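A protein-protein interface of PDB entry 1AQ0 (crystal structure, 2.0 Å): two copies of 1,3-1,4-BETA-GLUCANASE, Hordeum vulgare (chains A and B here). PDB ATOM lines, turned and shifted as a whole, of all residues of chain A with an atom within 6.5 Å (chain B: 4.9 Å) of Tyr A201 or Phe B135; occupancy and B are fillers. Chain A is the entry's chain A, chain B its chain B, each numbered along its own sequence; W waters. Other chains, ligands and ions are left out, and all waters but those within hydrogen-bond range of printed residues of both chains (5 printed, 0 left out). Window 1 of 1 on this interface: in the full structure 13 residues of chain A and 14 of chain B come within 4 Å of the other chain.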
ATOM      1  N   THR A 194     -18.386  -6.430  -1.800  1.00  0.00           N
ATOM      2  CA  THR A 194     -18.938  -5.096  -2.012  1.00  0.00           C
ATOM      3  C   THR A 194     -18.286  -4.386  -3.190  1.00  0.00           C
ATOM      4  O   THR A 194     -17.069  -4.196  -3.225  1.00  0.00           O
ATOM      5  CB  THR A 194     -18.739  -4.222  -0.760  1.00  0.00           C
ATOM      6  OG1 THR A 194     -19.304  -4.888   0.374  1.00  0.00           O
ATOM      7  CG2 THR A 194     -19.401  -2.861  -0.932  1.00  0.00           C
ATOM      8  N   VAL A 196     -19.991  -1.437  -4.573  1.00  0.00           N
ATOM      9  CA  VAL A 196     -20.316  -0.044  -4.321  1.00  0.00           C
ATOM     10  C   VAL A 196     -20.617   0.168  -2.847  1.00  0.00           C
ATOM     11  O   VAL A 196     -21.498  -0.487  -2.284  1.00  0.00           O
ATOM     12  CB  VAL A 196     -21.539   0.420  -5.159  1.00  0.00           C
ATOM     13  CG1 VAL A 196     -21.880   1.877  -4.855  1.00  0.00           C
ATOM     14  CG2 VAL A 196     -21.254   0.247  -6.641  1.00  0.00           C
ATOM     15  N   ARG A 197     -19.832   1.039  -2.220  1.00  0.00           N
ATOM     16  CA  ARG A 197     -20.001   1.395  -0.816  1.00  0.00           C
ATOM     17  C   ARG A 197     -20.741   2.734  -0.813  1.00  0.00           C
ATOM     18  O   ARG A 197     -20.254   3.728  -1.346  1.00  0.00           O
ATOM     19  CB  ARG A 197     -18.633   1.543  -0.143  1.00  0.00           C
ATOM     20  CG  ARG A 197     -18.665   1.517   1.380  1.00  0.00           C
ATOM     21  CD  ARG A 197     -19.227   0.190   1.884  1.00  0.00           C
ATOM     22  NE  ARG A 197     -18.836  -0.111   3.259  1.00  0.00           N
ATOM     23  CZ  ARG A 197     -19.192  -1.214   3.914  1.00  0.00           C
ATOM     24  NH1 ARG A 197     -20.181  -1.978   3.460  1.00  0.00           N
ATOM     25  NH2 ARG A 197     -18.532  -1.573   5.008  1.00  0.00           N
ATOM     26  N   ASP A 198     -21.928   2.751  -0.230  1.00  0.00           N
ATOM     27  CA  ASP A 198     -22.758   3.945  -0.187  1.00  0.00           C
ATOM     28  C   ASP A 198     -23.003   4.293   1.284  1.00  0.00           C
ATOM     29  O   ASP A 198     -23.993   3.864   1.881  1.00  0.00           O
ATOM     30  CB  ASP A 198     -24.071   3.630  -0.918  1.00  0.00           C
ATOM     31  CG  ASP A 198     -24.967   4.829  -1.078  1.00  0.00           C
ATOM     32  OD1 ASP A 198     -24.552   5.965  -0.779  1.00  0.00           O
ATOM     33  OD2 ASP A 198     -26.108   4.628  -1.522  1.00  0.00           O
ATOM     34  N   GLY A 199     -22.116   5.106   1.850  1.00  0.00           N
ATOM     35  CA  GLY A 199     -22.234   5.455   3.252  1.00  0.00           C
ATOM     36  C   GLY A 199     -21.873   4.193   4.010  1.00  0.00           C
ATOM     37  O   GLY A 199     -20.763   3.688   3.871  1.00  0.00           O
ATOM     38  N   ALA A 200     -22.833   3.637   4.739  1.00  0.00           N
ATOM     39  CA  ALA A 200     -22.618   2.411   5.503  1.00  0.00           C
ATOM     40  C   ALA A 200     -23.144   1.181   4.763  1.00  0.00           C
ATOM     41  O   ALA A 200     -22.954   0.052   5.215  1.00  0.00           O
ATOM     42  CB  ALA A 200     -23.311   2.518   6.849  1.00  0.00           C
ATOM     43  N   TYR A 201     -23.805   1.403   3.633  1.00  0.00           N
ATOM     44  CA  TYR A 201     -24.399   0.315   2.860  1.00  0.00           C
ATOM     45  C   TYR A 201     -23.513  -0.259   1.764  1.00  0.00           C
ATOM     46  O   TYR A 201     -22.793   0.470   1.092  1.00  0.00           O
ATOM     47  CB  TYR A 201     -25.741   0.780   2.305  1.00  0.00           C
ATOM     48  CG  TYR A 201     -26.641   1.307   3.402  1.00  0.00           C
ATOM     49  CD1 TYR A 201     -26.534   2.623   3.846  1.00  0.00           C
ATOM     50  CD2 TYR A 201     -27.560   0.471   4.036  1.00  0.00           C
ATOM     51  CE1 TYR A 201     -27.315   3.096   4.896  1.00  0.00           C
ATOM     52  CE2 TYR A 201     -28.347   0.933   5.082  1.00  0.00           C
ATOM     53  CZ  TYR A 201     -28.219   2.245   5.510  1.00  0.00           C
ATOM     54  OH  TYR A 201     -28.993   2.704   6.551  1.00  0.00           O
ATOM     55  N   GLY A 202     -23.556  -1.578   1.603  1.00  0.00           N
ATOM     56  CA  GLY A 202     -22.740  -2.233   0.591  1.00  0.00           C
ATOM     57  C   GLY A 202     -23.553  -2.929  -0.487  1.00  0.00           C
ATOM     58  O   GLY A 202     -24.464  -3.694  -0.186  1.00  0.00           O
ATOM     59  N   TYR A 203     -23.235  -2.655  -1.747  1.00  0.00           N
ATOM     60  CA  TYR A 203     -23.940  -3.267  -2.867  1.00  0.00           C
ATOM     61  C   TYR A 203     -22.993  -4.165  -3.644  1.00  0.00           C
ATOM     62  O   TYR A 203     -21.888  -3.750  -3.996  1.00  0.00           O
ATOM     63  CB  TYR A 203     -24.513  -2.190  -3.796  1.00  0.00           C
ATOM     64  CG  TYR A 203     -25.606  -1.372  -3.155  1.00  0.00           C
ATOM     65  CD1 TYR A 203     -25.300  -0.354  -2.253  1.00  0.00           C
ATOM     66  CD2 TYR A 203     -26.948  -1.661  -3.397  1.00  0.00           C
ATOM     67  CE1 TYR A 203     -26.298   0.342  -1.601  1.00  0.00           C
ATOM     68  CE2 TYR A 203     -27.954  -0.967  -2.755  1.00  0.00           C
ATOM     69  CZ  TYR A 203     -27.624   0.031  -1.855  1.00  0.00           C
ATOM     70  OH  TYR A 203     -28.619   0.710  -1.199  1.00  0.00           O
ATOM     71  N   PRO A 264     -30.185  -4.064   0.144  1.00  0.00           N
ATOM     72  CA  PRO A 264     -29.592  -3.512   1.367  1.00  0.00           C
ATOM     73  C   PRO A 264     -30.498  -2.534   2.132  1.00  0.00           C
ATOM     74  O   PRO A 264     -30.604  -2.623   3.352  1.00  0.00           O
ATOM     75  CB  PRO A 264     -28.331  -2.829   0.843  1.00  0.00           C
ATOM     76  CG  PRO A 264     -27.908  -3.750  -0.266  1.00  0.00           C
ATOM     77  CD  PRO A 264     -29.219  -3.999  -0.972  1.00  0.00           C
ATOM     78  N   ARG A 265     -31.141  -1.604   1.424  1.00  0.00           N
ATOM     79  CA  ARG A 265     -32.025  -0.623   2.065  1.00  0.00           C
ATOM     80  C   ARG A 265     -33.488  -1.043   2.107  1.00  0.00           C
ATOM     81  O   ARG A 265     -34.303  -0.405   2.769  1.00  0.00           O
ATOM     82  CB  ARG A 265     -31.910   0.753   1.390  1.00  0.00           C
ATOM     83  CG  ARG A 265     -30.629   1.511   1.717  1.00  0.00           C
ATOM     84  CD  ARG A 265     -30.591   2.846   0.991  1.00  0.00           C
ATOM     85  NE  ARG A 265     -29.549   3.722   1.513  1.00  0.00           N
ATOM     86  CZ  ARG A 265     -28.338   3.856   0.984  1.00  0.00           C
ATOM     87  NH1 ARG A 265     -27.990   3.166  -0.094  1.00  0.00           N
ATOM     88  NH2 ARG A 265     -27.487   4.729   1.509  1.00  0.00           N
ATOM     89  N   HIS A 266     -33.839  -2.080   1.362  1.00  0.00           N
ATOM     90  CA  HIS A 266     -35.213  -2.561   1.359  1.00  0.00           C
ATOM     91  C   HIS A 266     -35.271  -4.067   1.472  1.00  0.00           C
ATOM     92  O   HIS A 266     -35.502  -4.762   0.482  1.00  0.00           O
ATOM     93  CB  HIS A 266     -35.954  -2.074   0.106  1.00  0.00           C
ATOM     94  CG  HIS A 266     -36.115  -0.590   0.060  1.00  0.00           C
ATOM     95  ND1 HIS A 266     -35.139   0.252  -0.441  1.00  0.00           N
ATOM     96  CD2 HIS A 266     -37.083   0.219   0.548  1.00  0.00           C
ATOM     97  CE1 HIS A 266     -35.495   1.505  -0.248  1.00  0.00           C
ATOM     98  NE2 HIS A 266     -36.674   1.514   0.351  1.00  0.00           N
ATOM     99  N   PRO A 267     -34.988  -4.600   2.675  1.00  0.00           N
ATOM    100  CA  PRO A 267     -35.018  -6.045   2.901  1.00  0.00           C
ATOM    101  C   PRO A 267     -36.437  -6.576   2.733  1.00  0.00           C
ATOM    102  O   PRO A 267     -37.405  -5.857   2.972  1.00  0.00           O
ATOM    103  CB  PRO A 267     -34.514  -6.176   4.344  1.00  0.00           C
ATOM    104  CG  PRO A 267     -34.917  -4.885   4.972  1.00  0.00           C
ATOM    105  CD  PRO A 267     -34.570  -3.891   3.899  1.00  0.00           C
ATOM    106  N   LEU B 132     -41.480  -0.816   9.825  1.00  0.00           N
ATOM    107  CA  LEU B 132     -40.961   0.261   8.990  1.00  0.00           C
ATOM    108  C   LEU B 132     -40.691  -0.285   7.585  1.00  0.00           C
ATOM    109  O   LEU B 132     -39.960  -1.263   7.423  1.00  0.00           O
ATOM    110  CB  LEU B 132     -39.651   0.830   9.553  1.00  0.00           C
ATOM    111  CG  LEU B 132     -39.661   1.723  10.793  1.00  0.00           C
ATOM    112  CD1 LEU B 132     -38.247   2.177  11.082  1.00  0.00           C
ATOM    113  CD2 LEU B 132     -40.558   2.929  10.573  1.00  0.00           C
ATOM    114  N   GLY B 133     -41.311   0.323   6.582  1.00  0.00           N
ATOM    115  CA  GLY B 133     -41.091  -0.096   5.208  1.00  0.00           C
ATOM    116  C   GLY B 133     -39.808   0.532   4.695  1.00  0.00           C
ATOM    117  O   GLY B 133     -39.109  -0.035   3.852  1.00  0.00           O
ATOM    118  N   VAL B 134     -39.511   1.728   5.202  1.00  0.00           N
ATOM    119  CA  VAL B 134     -38.306   2.468   4.843  1.00  0.00           C
ATOM    120  C   VAL B 134     -37.688   3.055   6.113  1.00  0.00           C
ATOM    121  O   VAL B 134     -38.376   3.693   6.901  1.00  0.00           O
ATOM    122  CB  VAL B 134     -38.619   3.638   3.875  1.00  0.00           C
ATOM    123  CG1 VAL B 134     -37.362   4.477   3.635  1.00  0.00           C
ATOM    124  CG2 VAL B 134     -39.163   3.106   2.556  1.00  0.00           C
ATOM    125  N   PHE B 135     -36.402   2.814   6.325  1.00  0.00           N
ATOM    126  CA  PHE B 135     -35.725   3.350   7.497  1.00  0.00           C
ATOM    127  C   PHE B 135     -34.563   4.215   7.039  1.00  0.00           C
ATOM    128  O   PHE B 135     -34.098   5.091   7.761  1.00  0.00           O
ATOM    129  CB  PHE B 135     -35.236   2.217   8.420  1.00  0.00           C
ATOM    130  CG  PHE B 135     -34.205   1.309   7.794  1.00  0.00           C
ATOM    131  CD1 PHE B 135     -32.849   1.620   7.862  1.00  0.00           C
ATOM    132  CD2 PHE B 135     -34.592   0.143   7.138  1.00  0.00           C
ATOM    133  CE1 PHE B 135     -31.893   0.785   7.284  1.00  0.00           C
ATOM    134  CE2 PHE B 135     -33.639  -0.701   6.554  1.00  0.00           C
ATOM    135  CZ  PHE B 135     -32.287  -0.375   6.629  1.00  0.00           C
ATOM    136  N   SER B 136     -34.114   3.966   5.815  1.00  0.00           N
ATOM    137  CA  SER B 136     -32.998   4.698   5.234  1.00  0.00           C
ATOM    138  C   SER B 136     -33.384   5.289   3.871  1.00  0.00           C
ATOM    139  O   SER B 136     -33.814   4.555   2.977  1.00  0.00           O
ATOM    140  CB  SER B 136     -31.813   3.751   5.064  1.00  0.00           C
ATOM    141  OG  SER B 136     -30.721   4.400   4.443  1.00  0.00           O
ATOM    142  N   PRO B 137     -33.264   6.621   3.704  1.00  0.00           N
ATOM    143  CA  PRO B 137     -32.805   7.584   4.710  1.00  0.00           C
ATOM    144  C   PRO B 137     -33.956   7.925   5.658  1.00  0.00           C
ATOM    145  O   PRO B 137     -35.126   7.790   5.290  1.00  0.00           O
ATOM    146  CB  PRO B 137     -32.394   8.775   3.858  1.00  0.00           C
ATOM    147  CG  PRO B 137     -33.411   8.753   2.769  1.00  0.00           C
ATOM    148  CD  PRO B 137     -33.485   7.288   2.407  1.00  0.00           C
ATOM    149  N   PRO B 138     -33.644   8.386   6.882  1.00  0.00           N
ATOM    150  CA  PRO B 138     -34.668   8.736   7.875  1.00  0.00           C
ATOM    151  C   PRO B 138     -35.751   9.694   7.387  1.00  0.00           C
ATOM    152  O   PRO B 138     -36.909   9.558   7.760  1.00  0.00           O
ATOM    153  CB  PRO B 138     -33.850   9.358   9.000  1.00  0.00           C
ATOM    154  CG  PRO B 138     -32.553   8.660   8.904  1.00  0.00           C
ATOM    155  CD  PRO B 138     -32.295   8.632   7.419  1.00  0.00           C
ATOM    156  N   ALA B 181     -24.928  -6.235   3.557  1.00  0.00           N
ATOM    157  CA  ALA B 181     -25.653  -5.008   3.230  1.00  0.00           C
ATOM    158  C   ALA B 181     -25.169  -3.741   3.935  1.00  0.00           C
ATOM    159  O   ALA B 181     -25.405  -2.632   3.450  1.00  0.00           O
ATOM    160  CB  ALA B 181     -27.140  -5.206   3.472  1.00  0.00           C
ATOM    161  N   MET B 182     -24.536  -3.888   5.094  1.00  0.00           N
ATOM    162  CA  MET B 182     -24.039  -2.722   5.803  1.00  0.00           C
ATOM    163  C   MET B 182     -22.872  -3.040   6.703  1.00  0.00           C
ATOM    164  O   MET B 182     -22.675  -4.185   7.100  1.00  0.00           O
ATOM    165  CB  MET B 182     -25.153  -2.031   6.607  1.00  0.00           C
ATOM    166  CG  MET B 182     -25.781  -2.874   7.696  1.00  0.00           C
ATOM    167  SD  MET B 182     -26.868  -1.913   8.765  1.00  0.00           S
ATOM    168  CE  MET B 182     -28.369  -1.976   7.837  1.00  0.00           C
ATOM    169  N   TYR B 186     -21.544   0.268  11.888  1.00  0.00           N
ATOM    170  CA  TYR B 186     -22.676   1.196  11.842  1.00  0.00           C
ATOM    171  C   TYR B 186     -23.767   0.764  12.824  1.00  0.00           C
ATOM    172  O   TYR B 186     -24.408   1.597  13.469  1.00  0.00           O
ATOM    173  CB  TYR B 186     -23.238   1.257  10.418  1.00  0.00           C
ATOM    174  CG  TYR B 186     -24.194   2.406  10.139  1.00  0.00           C
ATOM    175  CD1 TYR B 186     -23.774   3.734  10.240  1.00  0.00           C
ATOM    176  CD2 TYR B 186     -25.502   2.161   9.716  1.00  0.00           C
ATOM    177  CE1 TYR B 186     -24.627   4.785   9.923  1.00  0.00           C
ATOM    178  CE2 TYR B 186     -26.364   3.210   9.397  1.00  0.00           C
ATOM    179  CZ  TYR B 186     -25.915   4.520   9.501  1.00  0.00           C
ATOM    180  OH  TYR B 186     -26.751   5.565   9.171  1.00  0.00           O
ATOM    181  N   VAL B 196     -23.274   9.188   7.227  1.00  0.00           N
ATOM    182  CA  VAL B 196     -24.247   9.000   6.161  1.00  0.00           C
ATOM    183  C   VAL B 196     -25.150  10.224   6.142  1.00  0.00           C
ATOM    184  O   VAL B 196     -25.925  10.470   7.070  1.00  0.00           O
ATOM    185  CB  VAL B 196     -25.066   7.697   6.345  1.00  0.00           C
ATOM    186  CG1 VAL B 196     -25.990   7.479   5.150  1.00  0.00           C
ATOM    187  CG2 VAL B 196     -24.123   6.508   6.496  1.00  0.00           C
ATOM    188  N   LEU B 206     -26.821   3.149  13.206  1.00  0.00           N
ATOM    189  CA  LEU B 206     -28.135   2.667  12.813  1.00  0.00           C
ATOM    190  C   LEU B 206     -29.229   2.964  13.834  1.00  0.00           C
ATOM    191  O   LEU B 206     -30.399   3.093  13.469  1.00  0.00           O
ATOM    192  CB  LEU B 206     -28.064   1.163  12.510  1.00  0.00           C
ATOM    193  CG  LEU B 206     -29.291   0.493  11.884  1.00  0.00           C
ATOM    194  CD1 LEU B 206     -29.742   1.252  10.639  1.00  0.00           C
ATOM    195  CD2 LEU B 206     -28.951  -0.947  11.540  1.00  0.00           C
ATOM    196  N   THR B 209     -30.614   6.419  13.070  1.00  0.00           N
ATOM    197  CA  THR B 209     -31.314   6.328  11.796  1.00  0.00           C
ATOM    198  C   THR B 209     -32.711   5.730  11.989  1.00  0.00           C
ATOM    199  O   THR B 209     -33.707   6.293  11.527  1.00  0.00           O
ATOM    200  CB  THR B 209     -30.497   5.467  10.800  1.00  0.00           C
ATOM    201  OG1 THR B 209     -29.235   6.097  10.555  1.00  0.00           O
ATOM    202  CG2 THR B 209     -31.230   5.294   9.482  1.00  0.00           C
ATOM    203  N   ALA B 213     -36.300   7.524  11.673  1.00  0.00           N
ATOM    204  CA  ALA B 213     -37.177   6.993  10.643  1.00  0.00           C
ATOM    205  C   ALA B 213     -38.562   6.810  11.258  1.00  0.00           C
ATOM    206  O   ALA B 213     -39.576   7.115  10.624  1.00  0.00           O
ATOM    207  CB  ALA B 213     -36.642   5.665  10.117  1.00  0.00           C
HETATM  208  O   HOH W   1     -28.849   6.949   3.053  1.00  0.00           O
HETATM  209  O   HOH W   2     -35.017   2.022   3.722  1.00  0.00           O
HETATM  210  O   HOH W   3     -36.522  -0.918   4.100  1.00  0.00           O
HETATM  211  O   HOH W   4     -38.472  -3.041   2.626  1.00  0.00           O
HETATM  212  O   HOH W   5     -35.067   4.358   0.373  1.00  0.00           O
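The backbone NH of Gly A202 sits at hydrogen-bond distance from the backbone carbonyl oxygen of Ala B181, 2.8 Å away.
OH of Tyr A201 sits at hydrogen-bond distance from OG of Ser B136.
The side-chain hydroxyl (OG) of Ser B136 lies within hydrogen-bond range of the guanidinium group (NE) of Arg A265.
Water W3 lies within hydrogen-bond range of the backbone carbonyl oxygen of Arg A265 (2.6 Å) and the backbone carbonyl oxygen of Gly B133 (2.7 Å).
Water W2 lies within hydrogen-bond range of the backbone carbonyl oxygen of Arg A265 (2.7 Å), the backbone carbonyl oxygen of Ser B136 (2.9 Å) and the backbone NH of Phe B135 (3.1 Å).
Water W5 lies within hydrogen-bond range of the backbone carbonyl oxygen (O) of Ser B136 and a ring nitrogen (NE2) of His A266.
Water W1 bridges the guanidinium group of Arg A265 (3.0 Å) and the side-chain hydroxyl of Ser B136 (3.5 Å).
Water W4 bridges O of Pro A267 and O of Gly B133.
Among the printed residues, pairs that only touch across the chains: Gly A199 with Val B196, Ala A200 with Met B182, Ala A200 with Tyr B186, Ala A200 with Val B196, Tyr A201 with Phe B135, Tyr A201 with Ala B181, Tyr A201 with Tyr B186, Pro A264 with Ala B181, Arg A265 with Phe B135, His A266 with Gly B133 and His A266 with Val B134.
Arg A197 touches none of the printed residues of chain B.
Printed residues of chain B within 4 Å of Gly A199: Val B196.
Of the printed residues of chain B, Ala A200 touches Met B182, Tyr B186 and Val B196.
Of the printed residues of chain B, Tyr A201 touches Phe B135 (3.6 Å), Ser B136 (3.2 Å), Ala B181 (3.2 Å) and Tyr B186 (3.9 Å).
Printed residues of chain A within 4 Å of Gly B133: His A266.
Of chain A, only Tyr A201 (3.6 Å) and Arg A265 (3.9 Å) come within 4 Å of Phe B135.
Printed residues of chain A within 4 Å of Ala B181: Tyr A201, Gly A202 and Pro A264.
Printed residues of chain A within 4 Å of Val B196: Gly A199 (3.9 Å) and Ala A200 (3.6 Å).
Leu B206 touches none of the printed residues of chain A.
The nearest residue of chain A that does not touch Phe B135 is Pro A267 (4.3 Å).
The nearest printed residue of chain A that does not touch Ala B181 is Ala A200 (4.04 Å).
Of the 14 printed residues of chain B, 8 touch a printed residue of chain A.
Hydrophobic or aromatic side chains of chain B within 4 Å of the printed part of chain A: Val B134, Phe B135, Ala B181, Met B182, Tyr B186 and Val B196.
Along chain B the printed residues that touch a printed residue of chain A span positions 133 to 196.
Of the 13 printed residues of chain A, 7 touch a printed residue of chain B.
Hydrophobic or aromatic side chains of chain A within 4 Å of the printed part of chain B: Ala A200, Tyr A201, Pro A264 and His A266.
Among the printed residues, no Asp or Glu carboxylate lies within 4 Å of a Lys or Arg side-chain nitrogen of the other chain.
The guanidinium group (NH1) of Arg A265 is in salt-bridge range of the side-chain carboxylate (OD2) of Asp A198 (2.8 Å).
OH of Tyr A203 is in hydrogen-bond range of NH1 of Arg A265.
N of Leu B206 is in hydrogen-bond range of O of Tyr B186.
OH of Tyr B186 lies within hydrogen-bond range of OG1 of Thr B209 (2.9 Å).
1 position is printed for both chains.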
